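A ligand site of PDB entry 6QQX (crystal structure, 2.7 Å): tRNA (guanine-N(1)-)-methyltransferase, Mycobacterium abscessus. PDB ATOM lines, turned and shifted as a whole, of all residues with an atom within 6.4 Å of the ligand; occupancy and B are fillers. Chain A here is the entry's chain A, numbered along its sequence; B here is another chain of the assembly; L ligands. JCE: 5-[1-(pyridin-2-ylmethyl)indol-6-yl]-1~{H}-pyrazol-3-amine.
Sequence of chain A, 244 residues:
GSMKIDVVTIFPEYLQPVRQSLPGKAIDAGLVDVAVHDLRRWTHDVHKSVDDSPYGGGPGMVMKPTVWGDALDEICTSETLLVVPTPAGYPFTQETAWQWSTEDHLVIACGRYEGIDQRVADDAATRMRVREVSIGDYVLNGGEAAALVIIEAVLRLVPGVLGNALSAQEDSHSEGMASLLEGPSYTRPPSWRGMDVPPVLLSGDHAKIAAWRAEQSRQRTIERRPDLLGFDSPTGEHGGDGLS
O of Tyr 138 sits close to N03 of the ligand. OG of Ser 134 is in hydrogen-bond range of N01 of the ligand. The backbone NH (N) of Leu 140 lies close to a nitrogen (N04) of the ligand (3.0 Å). A nitrogen (N01) of the ligand lies within hydrogen-bond range of the backbone carbonyl oxygen (O) of Gly 136 (3.3 Å).
The backbone carbonyl oxygen (O) of Ile 135 is in hydrogen-bond range of the side-chain hydroxyl (OH) of Tyr 138 (3.2 Å). The backbone carbonyl oxygen of Gly 136 is in hydrogen-bond range of the side-chain hydroxyl of Ser 134 (3.0 Å). The backbone carbonyl oxygen (O) of Gly 111 sits at hydrogen-bond distance from the backbone NH (N) of Gly 143. The side-chain sulfur (SG) of Cys 110 sits at hydrogen-bond distance from the backbone carbonyl oxygen (O) of Gly 143 (3.5 Å). The side-chain amide oxygen (OD1) of Asn 141 sits at hydrogen-bond distance from the guanidinium group (NE) of Arg 156 of chain B (3.3 Å). The side-chain hydroxyl (OG1) of Thr 86 lies close to the backbone NH (N) of Ala 88. NE of Arg 112 is in salt-bridge range of OE1 of Glu 144 (2.8 Å). NH1 of Arg 156 of chain B lies close to O of Val 139.
N of Ile 135 lies close to N01 of the ligand (3.1 Å). A nitrogen (N11) of the ligand lies close to the backbone carbonyl oxygen (O) of Asn 141 (3.5 Å). O of Pro 85 touches C08 of the ligand (3.3 Å). Thr 86 touches the ligand (C to C22, 3.5 Å). Pro 87 touches the ligand. Gly 111 touches the ligand (O to C20, 3.2 Å). Arg 112 touches the ligand. Tyr 113 touches the ligand (O to C12, 3.3 Å). Glu 114 touches the ligand (O to C15, 3.5 Å). Val 139 touches the ligand. C of Gly 142 touches C08 of the ligand, at 3.5 Å. N of Gly 143 touches C08 of the ligand, at 3.4 Å. Glu 182 of chain B touches the ligand (OE2 to C16, 3.5 Å). Of the 27 residues printed, 17 come within 4 Å of the ligand. The nearest printed residue that does not touch the ligand is Gly 115 (4.01 Å).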
ATOM      1  N   PRO A  85     -22.824   5.456 -11.177  1.00  0.00           N
ATOM      2  CA  PRO A  85     -23.901   6.449 -10.981  1.00  0.00           C
ATOM      3  C   PRO A  85     -23.362   7.883 -10.946  1.00  0.00           C
ATOM      4  O   PRO A  85     -22.344   8.156 -10.301  1.00  0.00           O
ATOM      5  CB  PRO A  85     -24.492   6.065  -9.630  1.00  0.00           C
ATOM      6  CG  PRO A  85     -24.211   4.600  -9.497  1.00  0.00           C
ATOM      7  CD  PRO A  85     -22.858   4.427 -10.117  1.00  0.00           C
ATOM      8  N   THR A  86     -24.042   8.764 -11.671  1.00  0.00           N
ATOM      9  CA  THR A  86     -23.654  10.176 -11.846  1.00  0.00           C
ATOM     10  C   THR A  86     -24.868  10.983 -12.345  1.00  0.00           C
ATOM     11  O   THR A  86     -25.663  10.464 -13.145  1.00  0.00           O
ATOM     12  CB  THR A  86     -22.423  10.350 -12.800  1.00  0.00           C
ATOM     13  OG1 THR A  86     -22.238  11.732 -13.130  1.00  0.00           O
ATOM     14  CG2 THR A  86     -22.565   9.533 -14.088  1.00  0.00           C
ATOM     15  N   PRO A  87     -25.032  12.250 -11.878  1.00  0.00           N
ATOM     16  CA  PRO A  87     -26.158  13.061 -12.375  1.00  0.00           C
ATOM     17  C   PRO A  87     -26.003  13.437 -13.854  1.00  0.00           C
ATOM     18  O   PRO A  87     -26.996  13.800 -14.494  1.00  0.00           O
ATOM     19  CB  PRO A  87     -26.119  14.309 -11.495  1.00  0.00           C
ATOM     20  CG  PRO A  87     -24.711  14.391 -10.992  1.00  0.00           C
ATOM     21  CD  PRO A  87     -24.254  12.973 -10.857  1.00  0.00           C
ATOM     22  N   ALA A  88     -24.783  13.335 -14.376  1.00  0.00           N
ATOM     23  CA  ALA A  88     -24.469  13.640 -15.771  1.00  0.00           C
ATOM     24  C   ALA A  88     -24.411  12.397 -16.671  1.00  0.00           C
ATOM     25  O   ALA A  88     -23.838  12.444 -17.751  1.00  0.00           O
ATOM     26  CB  ALA A  88     -23.171  14.418 -15.840  1.00  0.00           C
ATOM     27  N   ALA A 109     -19.690   1.501  -8.786  1.00  0.00           N
ATOM     28  CA  ALA A 109     -18.758   2.445  -8.175  1.00  0.00           C
ATOM     29  C   ALA A 109     -19.525   3.650  -7.630  1.00  0.00           C
ATOM     30  O   ALA A 109     -19.986   4.501  -8.386  1.00  0.00           O
ATOM     31  CB  ALA A 109     -17.712   2.882  -9.192  1.00  0.00           C
ATOM     32  N   CYS A 110     -19.663   3.692  -6.298  1.00  0.00           N
ATOM     33  CA  CYS A 110     -20.416   4.760  -5.629  1.00  0.00           C
ATOM     34  C   CYS A 110     -19.513   5.914  -5.207  1.00  0.00           C
ATOM     35  O   CYS A 110     -18.697   5.774  -4.289  1.00  0.00           O
ATOM     36  CB  CYS A 110     -21.200   4.215  -4.441  1.00  0.00           C
ATOM     37  SG  CYS A 110     -22.453   3.010  -4.904  1.00  0.00           S
ATOM     38  N   GLY A 111     -19.669   7.028  -5.890  1.00  0.00           N
ATOM     39  CA  GLY A 111     -18.923   8.243  -5.599  1.00  0.00           C
ATOM     40  C   GLY A 111     -19.607   9.124  -4.563  1.00  0.00           C
ATOM     41  O   GLY A 111     -20.793   8.944  -4.271  1.00  0.00           O
ATOM     42  N   ARG A 112     -18.830  10.054  -4.015  1.00  0.00           N
ATOM     43  CA  ARG A 112     -19.345  11.106  -3.135  1.00  0.00           C
ATOM     44  C   ARG A 112     -18.757  12.449  -3.568  1.00  0.00           C
ATOM     45  O   ARG A 112     -18.092  12.532  -4.608  1.00  0.00           O
ATOM     46  CB  ARG A 112     -19.026  10.783  -1.671  1.00  0.00           C
ATOM     47  CG  ARG A 112     -19.994   9.797  -1.023  1.00  0.00           C
ATOM     48  CD  ARG A 112     -21.172  10.504  -0.372  1.00  0.00           C
ATOM     49  NE  ARG A 112     -22.328   9.622  -0.257  1.00  0.00           N
ATOM     50  CZ  ARG A 112     -23.466   9.927   0.365  1.00  0.00           C
ATOM     51  NH1 ARG A 112     -23.624  11.120   0.947  1.00  0.00           N
ATOM     52  NH2 ARG A 112     -24.453   9.045   0.400  1.00  0.00           N
ATOM     53  N   TYR A 113     -19.014  13.487  -2.762  1.00  0.00           N
ATOM     54  CA  TYR A 113     -18.536  14.856  -3.008  1.00  0.00           C
ATOM     55  C   TYR A 113     -19.083  15.403  -4.337  1.00  0.00           C
ATOM     56  O   TYR A 113     -20.299  15.414  -4.536  1.00  0.00           O
ATOM     57  CB  TYR A 113     -16.996  14.955  -2.892  1.00  0.00           C
ATOM     58  CG  TYR A 113     -16.426  14.426  -1.591  1.00  0.00           C
ATOM     59  CD1 TYR A 113     -16.312  15.253  -0.463  1.00  0.00           C
ATOM     60  CD2 TYR A 113     -15.993  13.098  -1.475  1.00  0.00           C
ATOM     61  CE1 TYR A 113     -15.796  14.770   0.738  1.00  0.00           C
ATOM     62  CE2 TYR A 113     -15.472  12.604  -0.277  1.00  0.00           C
ATOM     63  CZ  TYR A 113     -15.372  13.446   0.821  1.00  0.00           C
ATOM     64  OH  TYR A 113     -14.861  12.966   2.005  1.00  0.00           O
ATOM     65  N   GLU A 114     -18.208  15.835  -5.251  1.00  0.00           N
ATOM     66  CA  GLU A 114     -18.632  16.322  -6.577  1.00  0.00           C
ATOM     67  C   GLU A 114     -18.440  15.279  -7.685  1.00  0.00           C
ATOM     68  O   GLU A 114     -18.591  15.575  -8.871  1.00  0.00           O
ATOM     69  CB  GLU A 114     -17.920  17.640  -6.926  1.00  0.00           C
ATOM     70  CG  GLU A 114     -18.265  18.820  -6.026  1.00  0.00           C
ATOM     71  CD  GLU A 114     -19.640  19.405  -6.282  1.00  0.00           C
ATOM     72  OE1 GLU A 114     -20.511  19.296  -5.384  1.00  0.00           O
ATOM     73  OE2 GLU A 114     -19.863  19.968  -7.380  1.00  0.00           O
ATOM     74  N   GLY A 115     -18.133  14.042  -7.279  1.00  0.00           N
ATOM     75  CA  GLY A 115     -17.931  12.933  -8.205  1.00  0.00           C
ATOM     76  C   GLY A 115     -16.535  12.351  -8.177  1.00  0.00           C
ATOM     77  O   GLY A 115     -15.717  12.717  -7.330  1.00  0.00           O
ATOM     78  N   ILE A 116     -16.273  11.455  -9.117  1.00  0.00           N
ATOM     79  CA  ILE A 116     -14.982  10.773  -9.253  1.00  0.00           C
ATOM     80  C   ILE A 116     -14.201  11.396 -10.408  1.00  0.00           C
ATOM     81  O   ILE A 116     -14.795  11.828 -11.402  1.00  0.00           O
ATOM     82  CB  ILE A 116     -15.180   9.234  -9.485  1.00  0.00           C
ATOM     83  CG1 ILE A 116     -16.153   8.642  -8.452  1.00  0.00           C
ATOM     84  CG2 ILE A 116     -13.844   8.497  -9.448  1.00  0.00           C
ATOM     85  CD1 ILE A 116     -16.843   7.362  -8.885  1.00  0.00           C
ATOM     86  N   VAL A 133     -24.400   6.272 -15.552  1.00  0.00           N
ATOM     87  CA  VAL A 133     -25.873   6.328 -15.540  1.00  0.00           C
ATOM     88  C   VAL A 133     -26.503   7.300 -14.531  1.00  0.00           C
ATOM     89  O   VAL A 133     -25.949   7.531 -13.452  1.00  0.00           O
ATOM     90  CB  VAL A 133     -26.531   4.919 -15.366  1.00  0.00           C
ATOM     91  CG1 VAL A 133     -26.344   4.073 -16.623  1.00  0.00           C
ATOM     92  CG2 VAL A 133     -26.005   4.198 -14.126  1.00  0.00           C
ATOM     93  N   SER A 134     -27.646   7.860 -14.905  1.00  0.00           N
ATOM     94  CA  SER A 134     -28.492   8.668 -14.034  1.00  0.00           C
ATOM     95  C   SER A 134     -29.828   7.970 -13.813  1.00  0.00           C
ATOM     96  O   SER A 134     -30.434   7.460 -14.757  1.00  0.00           O
ATOM     97  CB  SER A 134     -28.715  10.053 -14.636  1.00  0.00           C
ATOM     98  OG  SER A 134     -29.700  10.792 -13.923  1.00  0.00           O
ATOM     99  N   ILE A 135     -30.274   7.943 -12.559  1.00  0.00           N
ATOM    100  CA  ILE A 135     -31.554   7.316 -12.189  1.00  0.00           C
ATOM    101  C   ILE A 135     -32.754   8.274 -12.288  1.00  0.00           C
ATOM    102  O   ILE A 135     -33.907   7.858 -12.153  1.00  0.00           O
ATOM    103  CB  ILE A 135     -31.513   6.613 -10.795  1.00  0.00           C
ATOM    104  CG1 ILE A 135     -31.167   7.595  -9.666  1.00  0.00           C
ATOM    105  CG2 ILE A 135     -30.537   5.423 -10.827  1.00  0.00           C
ATOM    106  CD1 ILE A 135     -31.727   7.209  -8.306  1.00  0.00           C
ATOM    107  N   GLY A 136     -32.473   9.556 -12.548  1.00  0.00           N
ATOM    108  CA  GLY A 136     -33.512  10.587 -12.686  1.00  0.00           C
ATOM    109  C   GLY A 136     -32.978  12.006 -12.694  1.00  0.00           C
ATOM    110  O   GLY A 136     -31.796  12.236 -12.421  1.00  0.00           O
ATOM    111  N   ASP A 137     -33.861  12.956 -13.004  1.00  0.00           N
ATOM    112  CA  ASP A 137     -33.509  14.385 -13.095  1.00  0.00           C
ATOM    113  C   ASP A 137     -33.549  15.093 -11.737  1.00  0.00           C
ATOM    114  O   ASP A 137     -34.309  16.046 -11.526  1.00  0.00           O
ATOM    115  CB  ASP A 137     -34.398  15.101 -14.129  1.00  0.00           C
ATOM    116  CG  ASP A 137     -34.142  14.623 -15.551  1.00  0.00           C
ATOM    117  OD1 ASP A 137     -33.277  13.745 -15.757  1.00  0.00           O
ATOM    118  OD2 ASP A 137     -34.810  15.145 -16.473  1.00  0.00           O
ATOM    119  N   TYR A 138     -32.708  14.603 -10.826  1.00  0.00           N
ATOM    120  CA  TYR A 138     -32.511  15.169  -9.499  1.00  0.00           C
ATOM    121  C   TYR A 138     -31.065  14.905  -9.091  1.00  0.00           C
ATOM    122  O   TYR A 138     -30.387  14.072  -9.681  1.00  0.00           O
ATOM    123  CB  TYR A 138     -33.489  14.539  -8.481  1.00  0.00           C
ATOM    124  CG  TYR A 138     -33.749  13.065  -8.677  1.00  0.00           C
ATOM    125  CD1 TYR A 138     -32.803  12.111  -8.288  1.00  0.00           C
ATOM    126  CD2 TYR A 138     -34.933  12.622  -9.264  1.00  0.00           C
ATOM    127  CE1 TYR A 138     -33.030  10.751  -8.485  1.00  0.00           C
ATOM    128  CE2 TYR A 138     -35.182  11.267  -9.460  1.00  0.00           C
ATOM    129  CZ  TYR A 138     -34.226  10.333  -9.066  1.00  0.00           C
ATOM    130  OH  TYR A 138     -34.458   8.992  -9.253  1.00  0.00           O
ATOM    131  N   VAL A 139     -30.603  15.634  -8.077  1.00  0.00           N
ATOM    132  CA  VAL A 139     -29.226  15.476  -7.583  1.00  0.00           C
ATOM    133  C   VAL A 139     -29.267  14.926  -6.156  1.00  0.00           C
ATOM    134  O   VAL A 139     -29.918  15.496  -5.268  1.00  0.00           O
ATOM    135  CB  VAL A 139     -28.409  16.797  -7.671  1.00  0.00           C
ATOM    136  CG1 VAL A 139     -26.958  16.571  -7.277  1.00  0.00           C
ATOM    137  CG2 VAL A 139     -28.470  17.379  -9.074  1.00  0.00           C
ATOM    138  N   LEU A 140     -28.604  13.783  -5.963  1.00  0.00           N
ATOM    139  CA  LEU A 140     -28.406  13.162  -4.648  1.00  0.00           C
ATOM    140  C   LEU A 140     -27.065  13.631  -4.075  1.00  0.00           C
ATOM    141  O   LEU A 140     -26.366  14.436  -4.699  1.00  0.00           O
ATOM    142  CB  LEU A 140     -28.449  11.631  -4.764  1.00  0.00           C
ATOM    143  CG  LEU A 140     -29.645  10.917  -5.423  1.00  0.00           C
ATOM    144  CD1 LEU A 140     -29.210   9.554  -5.936  1.00  0.00           C
ATOM    145  CD2 LEU A 140     -30.834  10.783  -4.481  1.00  0.00           C
ATOM    146  N   ASN A 141     -26.713  13.141  -2.881  1.00  0.00           N
ATOM    147  CA  ASN A 141     -25.417  13.440  -2.268  1.00  0.00           C
ATOM    148  C   ASN A 141     -24.302  12.481  -2.687  1.00  0.00           C
ATOM    149  O   ASN A 141     -23.121  12.828  -2.627  1.00  0.00           O
ATOM    150  CB  ASN A 141     -25.532  13.508  -0.740  1.00  0.00           C
ATOM    151  CG  ASN A 141     -25.932  14.882  -0.235  1.00  0.00           C
ATOM    152  OD1 ASN A 141     -25.408  15.905  -0.685  1.00  0.00           O
ATOM    153  ND2 ASN A 141     -26.843  14.909   0.720  1.00  0.00           N
ATOM    154  N   GLY A 142     -24.702  11.278  -3.108  1.00  0.00           N
ATOM    155  CA  GLY A 142     -23.776  10.250  -3.594  1.00  0.00           C
ATOM    156  C   GLY A 142     -24.458   9.214  -4.468  1.00  0.00           C
ATOM    157  O   GLY A 142     -25.638   9.340  -4.795  1.00  0.00           O
ATOM    158  N   GLY A 143     -23.708   8.177  -4.844  1.00  0.00           N
ATOM    159  CA  GLY A 143     -24.213   7.113  -5.707  1.00  0.00           C
ATOM    160  C   GLY A 143     -24.840   5.933  -4.997  1.00  0.00           C
ATOM    161  O   GLY A 143     -25.285   4.991  -5.644  1.00  0.00           O
ATOM    162  N   GLU A 144     -24.891   5.994  -3.667  1.00  0.00           N
ATOM    163  CA  GLU A 144     -25.355   4.892  -2.815  1.00  0.00           C
ATOM    164  C   GLU A 144     -26.859   4.602  -2.970  1.00  0.00           C
ATOM    165  O   GLU A 144     -27.254   3.441  -3.099  1.00  0.00           O
ATOM    166  CB  GLU A 144     -25.005   5.134  -1.345  1.00  0.00           C
ATOM    167  CG  GLU A 144     -23.528   4.982  -0.997  1.00  0.00           C
ATOM    168  CD  GLU A 144     -22.681   6.190  -1.352  1.00  0.00           C
ATOM    169  OE1 GLU A 144     -23.221   7.308  -1.490  1.00  0.00           O
ATOM    170  OE2 GLU A 144     -21.447   6.029  -1.482  1.00  0.00           O
ATOM    171  N   ALA A 146     -28.634   5.617  -5.538  1.00  0.00           N
ATOM    172  CA  ALA A 146     -28.708   5.221  -6.943  1.00  0.00           C
ATOM    173  C   ALA A 146     -28.399   3.741  -7.143  1.00  0.00           C
ATOM    174  O   ALA A 146     -29.036   3.079  -7.965  1.00  0.00           O
ATOM    175  CB  ALA A 146     -27.782   6.084  -7.793  1.00  0.00           C
ATOM    176  N   ARG B 156     -30.885  17.715   1.188  1.00  0.00           N
ATOM    177  CA  ARG B 156     -29.669  18.456   0.812  1.00  0.00           C
ATOM    178  C   ARG B 156     -29.952  19.874   0.314  1.00  0.00           C
ATOM    179  O   ARG B 156     -29.023  20.678   0.122  1.00  0.00           O
ATOM    180  CB  ARG B 156     -28.815  17.653  -0.193  1.00  0.00           C
ATOM    181  CG  ARG B 156     -29.419  17.499  -1.580  1.00  0.00           C
ATOM    182  CD  ARG B 156     -28.524  16.666  -2.485  1.00  0.00           C
ATOM    183  NE  ARG B 156     -27.329  17.384  -2.936  1.00  0.00           N
ATOM    184  CZ  ARG B 156     -27.291  18.237  -3.966  1.00  0.00           C
ATOM    185  NH1 ARG B 156     -28.373  18.502  -4.685  1.00  0.00           N
ATOM    186  NH2 ARG B 156     -26.146  18.817  -4.289  1.00  0.00           N
ATOM    187  N   GLU B 182     -23.416  18.064 -15.813  1.00  0.00           N
ATOM    188  CA  GLU B 182     -22.102  18.423 -15.276  1.00  0.00           C
ATOM    189  C   GLU B 182     -20.963  17.890 -16.148  1.00  0.00           C
ATOM    190  O   GLU B 182     -21.009  16.746 -16.617  1.00  0.00           O
ATOM    191  CB  GLU B 182     -21.942  17.923 -13.841  1.00  0.00           C
ATOM    192  CG  GLU B 182     -22.785  18.661 -12.811  1.00  0.00           C
ATOM    193  CD  GLU B 182     -22.067  19.833 -12.152  1.00  0.00           C
ATOM    194  OE1 GLU B 182     -21.282  20.541 -12.828  1.00  0.00           O
ATOM    195  OE2 GLU B 182     -22.291  20.057 -10.943  1.00  0.00           O
HETATM  196  C10 JCE L   1     -23.507  12.188  -6.804  1.00  0.00           C
HETATM  197  C13 JCE L   1     -22.933  15.471  -6.769  1.00  0.00           C
HETATM  198  C15 JCE L   1     -22.074  15.997  -8.893  1.00  0.00           C
HETATM  199  C17 JCE L   1     -23.054  17.778  -7.550  1.00  0.00           C
HETATM  200  C20 JCE L   1     -21.490  11.318  -6.329  1.00  0.00           C
HETATM  201  C21 JCE L   1     -24.835  12.230  -7.349  1.00  0.00           C
HETATM  202  C22 JCE L   1     -27.179  10.559  -9.802  1.00  0.00           C
HETATM  203  N01 JCE L   1     -29.377  10.467 -11.025  1.00  0.00           N
HETATM  204  C02 JCE L   1     -28.517  10.898  -9.971  1.00  0.00           C
HETATM  205  N03 JCE L   1     -28.863  11.709  -8.953  1.00  0.00           N
HETATM  206  N04 JCE L   1     -27.754  11.872  -8.177  1.00  0.00           N
HETATM  207  C05 JCE L   1     -26.745  11.186  -8.661  1.00  0.00           C
HETATM  208  C06 JCE L   1     -25.339  11.122  -8.067  1.00  0.00           C
HETATM  209  C07 JCE L   1     -24.535   9.975  -8.254  1.00  0.00           C
HETATM  210  C08 JCE L   1     -23.241   9.928  -7.725  1.00  0.00           C
HETATM  211  C09 JCE L   1     -22.725  11.046  -6.990  1.00  0.00           C
HETATM  212  N11 JCE L   1     -22.769  13.100  -6.068  1.00  0.00           N
HETATM  213  C12 JCE L   1     -23.211  14.421  -5.660  1.00  0.00           C
HETATM  214  N14 JCE L   1     -22.337  15.108  -7.912  1.00  0.00           N
HETATM  215  C16 JCE L   1     -22.418  17.337  -8.754  1.00  0.00           C
HETATM  216  C18 JCE L   1     -23.310  16.803  -6.533  1.00  0.00           C
HETATM  217  C19 JCE L   1     -21.566  12.600  -5.781  1.00  0.00           C
